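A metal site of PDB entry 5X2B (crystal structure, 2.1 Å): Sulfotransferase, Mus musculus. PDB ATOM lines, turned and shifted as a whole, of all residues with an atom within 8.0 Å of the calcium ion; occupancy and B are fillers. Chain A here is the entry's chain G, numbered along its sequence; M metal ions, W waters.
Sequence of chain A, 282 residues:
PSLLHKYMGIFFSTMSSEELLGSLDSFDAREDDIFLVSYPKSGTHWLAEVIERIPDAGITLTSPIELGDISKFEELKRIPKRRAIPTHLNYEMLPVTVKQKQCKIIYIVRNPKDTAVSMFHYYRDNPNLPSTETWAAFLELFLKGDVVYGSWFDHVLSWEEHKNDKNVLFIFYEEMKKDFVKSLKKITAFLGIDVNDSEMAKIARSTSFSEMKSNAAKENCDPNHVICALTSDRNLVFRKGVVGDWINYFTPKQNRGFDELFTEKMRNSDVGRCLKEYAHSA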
ATOM      1  N   ILE A 105     -16.524   5.727   1.029  1.00  0.00           N
ATOM      2  CA  ILE A 105     -17.192   4.961   2.078  1.00  0.00           C
ATOM      3  C   ILE A 105     -18.542   5.558   2.314  1.00  0.00           C
ATOM      4  O   ILE A 105     -18.633   6.771   2.476  1.00  0.00           O
ATOM      5  CB  ILE A 105     -16.552   5.142   3.444  1.00  0.00           C
ATOM      6  CG1 ILE A 105     -15.041   5.059   3.352  1.00  0.00           C
ATOM      7  CG2 ILE A 105     -17.139   4.135   4.453  1.00  0.00           C
ATOM      8  CD1 ILE A 105     -14.573   3.734   2.936  1.00  0.00           C
ATOM      9  N   HIS A 162     -14.320  10.433  11.429  1.00  0.00           N
ATOM     10  CA  HIS A 162     -13.999  10.556  10.007  1.00  0.00           C
ATOM     11  C   HIS A 162     -15.059  10.993   9.084  1.00  0.00           C
ATOM     12  O   HIS A 162     -14.985  10.714   7.889  1.00  0.00           O
ATOM     13  CB  HIS A 162     -13.447   9.253   9.449  1.00  0.00           C
ATOM     14  CG  HIS A 162     -12.096   8.995   9.953  1.00  0.00           C
ATOM     15  ND1 HIS A 162     -11.006   9.745   9.554  1.00  0.00           N
ATOM     16  CD2 HIS A 162     -11.657   8.213  10.980  1.00  0.00           C
ATOM     17  CE1 HIS A 162      -9.953   9.392  10.259  1.00  0.00           C
ATOM     18  NE2 HIS A 162     -10.331   8.469  11.119  1.00  0.00           N
ATOM     19  N   LYS A 163     -16.048  11.700   9.611  1.00  0.00           N
ATOM     20  CA  LYS A 163     -17.062  12.266   8.744  1.00  0.00           C
ATOM     21  C   LYS A 163     -16.551  13.431   7.881  1.00  0.00           C
ATOM     22  O   LYS A 163     -17.145  13.699   6.847  1.00  0.00           O
ATOM     23  CB  LYS A 163     -18.315  12.649   9.544  1.00  0.00           C
ATOM     24  CG  LYS A 163     -19.278  13.543   8.738  1.00  0.00           C
ATOM     25  CD  LYS A 163     -20.764  13.379   9.084  1.00  0.00           C
ATOM     26  CE  LYS A 163     -21.453  14.697   9.465  1.00  0.00           C
ATOM     27  NZ  LYS A 163     -21.943  15.468   8.287  1.00  0.00           N
ATOM     28  N   ASN A 164     -15.436  14.091   8.243  1.00  0.00           N
ATOM     29  CA  ASN A 164     -14.915  15.227   7.433  1.00  0.00           C
ATOM     30  C   ASN A 164     -13.962  14.922   6.319  1.00  0.00           C
ATOM     31  O   ASN A 164     -13.474  15.853   5.674  1.00  0.00           O
ATOM     32  CB  ASN A 164     -14.085  16.168   8.265  1.00  0.00           C
ATOM     33  CG  ASN A 164     -14.868  16.868   9.313  1.00  0.00           C
ATOM     34  OD1 ASN A 164     -16.111  16.935   9.244  1.00  0.00           O
ATOM     35  ND2 ASN A 164     -14.170  17.430  10.306  1.00  0.00           N
ATOM     36  N   ASP A 165     -13.578  13.669   6.158  1.00  0.00           N
ATOM     37  CA  ASP A 165     -12.690  13.269   5.082  1.00  0.00           C
ATOM     38  C   ASP A 165     -13.492  13.327   3.835  1.00  0.00           C
ATOM     39  O   ASP A 165     -14.650  12.945   3.813  1.00  0.00           O
ATOM     40  CB  ASP A 165     -12.242  11.838   5.232  1.00  0.00           C
ATOM     41  CG  ASP A 165     -11.463  11.608   6.448  1.00  0.00           C
ATOM     42  OD1 ASP A 165     -11.396  12.479   7.318  1.00  0.00           O
ATOM     43  OD2 ASP A 165     -10.941  10.488   6.539  1.00  0.00           O
ATOM     44  N   LYS A 166     -12.843  13.748   2.778  1.00  0.00           N
ATOM     45  CA  LYS A 166     -13.499  14.033   1.539  1.00  0.00           C
ATOM     46  C   LYS A 166     -14.188  12.803   0.965  1.00  0.00           C
ATOM     47  O   LYS A 166     -15.180  12.897   0.242  1.00  0.00           O
ATOM     48  CB  LYS A 166     -12.471  14.583   0.564  1.00  0.00           C
ATOM     49  CG  LYS A 166     -11.368  13.617   0.200  1.00  0.00           C
ATOM     50  CD  LYS A 166     -10.248  14.354  -0.534  1.00  0.00           C
ATOM     51  CE  LYS A 166      -9.271  13.401  -1.132  1.00  0.00           C
ATOM     52  NZ  LYS A 166      -9.872  12.753  -2.333  1.00  0.00           N
ATOM     53  N   ASN A 167     -13.690  11.638   1.312  1.00  0.00           N
ATOM     54  CA  ASN A 167     -14.123  10.424   0.666  1.00  0.00           C
ATOM     55  C   ASN A 167     -15.110   9.659   1.545  1.00  0.00           C
ATOM     56  O   ASN A 167     -15.547   8.549   1.221  1.00  0.00           O
ATOM     57  CB  ASN A 167     -12.906   9.575   0.350  1.00  0.00           C
ATOM     58  CG  ASN A 167     -12.022   9.414   1.547  1.00  0.00           C
ATOM     59  OD1 ASN A 167     -11.318  10.346   1.942  1.00  0.00           O
ATOM     60  ND2 ASN A 167     -12.095   8.259   2.165  1.00  0.00           N
ATOM     61  N   VAL A 168     -15.464  10.250   2.663  1.00  0.00           N
ATOM     62  CA  VAL A 168     -16.441   9.689   3.549  1.00  0.00           C
ATOM     63  C   VAL A 168     -17.758  10.493   3.545  1.00  0.00           C
ATOM     64  O   VAL A 168     -17.710  11.711   3.671  1.00  0.00           O
ATOM     65  CB  VAL A 168     -15.897   9.703   4.965  1.00  0.00           C
ATOM     66  CG1 VAL A 168     -16.944   9.261   5.943  1.00  0.00           C
ATOM     67  CG2 VAL A 168     -14.653   8.838   5.044  1.00  0.00           C
ATOM     68  N   LEU A 169     -18.898   9.807   3.427  1.00  0.00           N
ATOM     69  CA  LEU A 169     -20.253  10.404   3.526  1.00  0.00           C
ATOM     70  C   LEU A 169     -21.158   9.669   4.546  1.00  0.00           C
ATOM     71  O   LEU A 169     -21.263   8.460   4.485  1.00  0.00           O
ATOM     72  CB  LEU A 169     -20.943  10.359   2.157  1.00  0.00           C
ATOM     73  CG  LEU A 169     -22.371  10.918   1.931  1.00  0.00           C
ATOM     74  CD1 LEU A 169     -22.400  12.429   1.753  1.00  0.00           C
ATOM     75  CD2 LEU A 169     -22.974  10.263   0.714  1.00  0.00           C
ATOM     76  N   PHE A 170     -21.788  10.414   5.454  1.00  0.00           N
ATOM     77  CA  PHE A 170     -22.731   9.867   6.412  1.00  0.00           C
ATOM     78  C   PHE A 170     -24.129  10.007   5.934  1.00  0.00           C
ATOM     79  O   PHE A 170     -24.487  11.036   5.382  1.00  0.00           O
ATOM     80  CB  PHE A 170     -22.638  10.566   7.774  1.00  0.00           C
ATOM     81  CG  PHE A 170     -21.742   9.844   8.745  1.00  0.00           C
ATOM     82  CD1 PHE A 170     -20.444   9.551   8.416  1.00  0.00           C
ATOM     83  CD2 PHE A 170     -22.205   9.449   9.977  1.00  0.00           C
ATOM     84  CE1 PHE A 170     -19.635   8.874   9.311  1.00  0.00           C
ATOM     85  CE2 PHE A 170     -21.396   8.790  10.858  1.00  0.00           C
ATOM     86  CZ  PHE A 170     -20.114   8.499  10.524  1.00  0.00           C
ATOM     87  N   PHE A 190     -22.353  12.157  -4.285  1.00  0.00           N
ATOM     88  CA  PHE A 190     -21.101  11.730  -3.642  1.00  0.00           C
ATOM     89  C   PHE A 190     -20.351  10.704  -4.454  1.00  0.00           C
ATOM     90  O   PHE A 190     -19.136  10.787  -4.627  1.00  0.00           O
ATOM     91  CB  PHE A 190     -21.374  11.113  -2.264  1.00  0.00           C
ATOM     92  CG  PHE A 190     -20.146  10.553  -1.574  1.00  0.00           C
ATOM     93  CD1 PHE A 190     -19.111  11.395  -1.162  1.00  0.00           C
ATOM     94  CD2 PHE A 190     -20.064   9.197  -1.274  1.00  0.00           C
ATOM     95  CE1 PHE A 190     -18.008  10.858  -0.472  1.00  0.00           C
ATOM     96  CE2 PHE A 190     -18.962   8.672  -0.577  1.00  0.00           C
ATOM     97  CZ  PHE A 190     -17.931   9.501  -0.197  1.00  0.00           C
HETATM   98 CA    CA M   1     -16.890  13.767   4.041  1.00  0.00          CA
HETATM   99  O   HOH W   1     -16.808  14.386   1.856  1.00  0.00           O
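The calcium ion is bound by O of Val 168, water W1, O of Asp 165 and O of Lys 163. The calcium ion has four donor atoms within binding distance.
Merely in contact with the calcium ion: Asn 164 (3.9 Å). Of the 11 residues printed, 4 come within 4 Å of the calcium ion. The nearest printed residue that does not touch the calcium ion is Lys 166 (4.2 Å).
The side-chain carboxylate of Asp 165 is in hydrogen-bond range of a ring nitrogen (ND1) of His 162 (3.1 Å).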
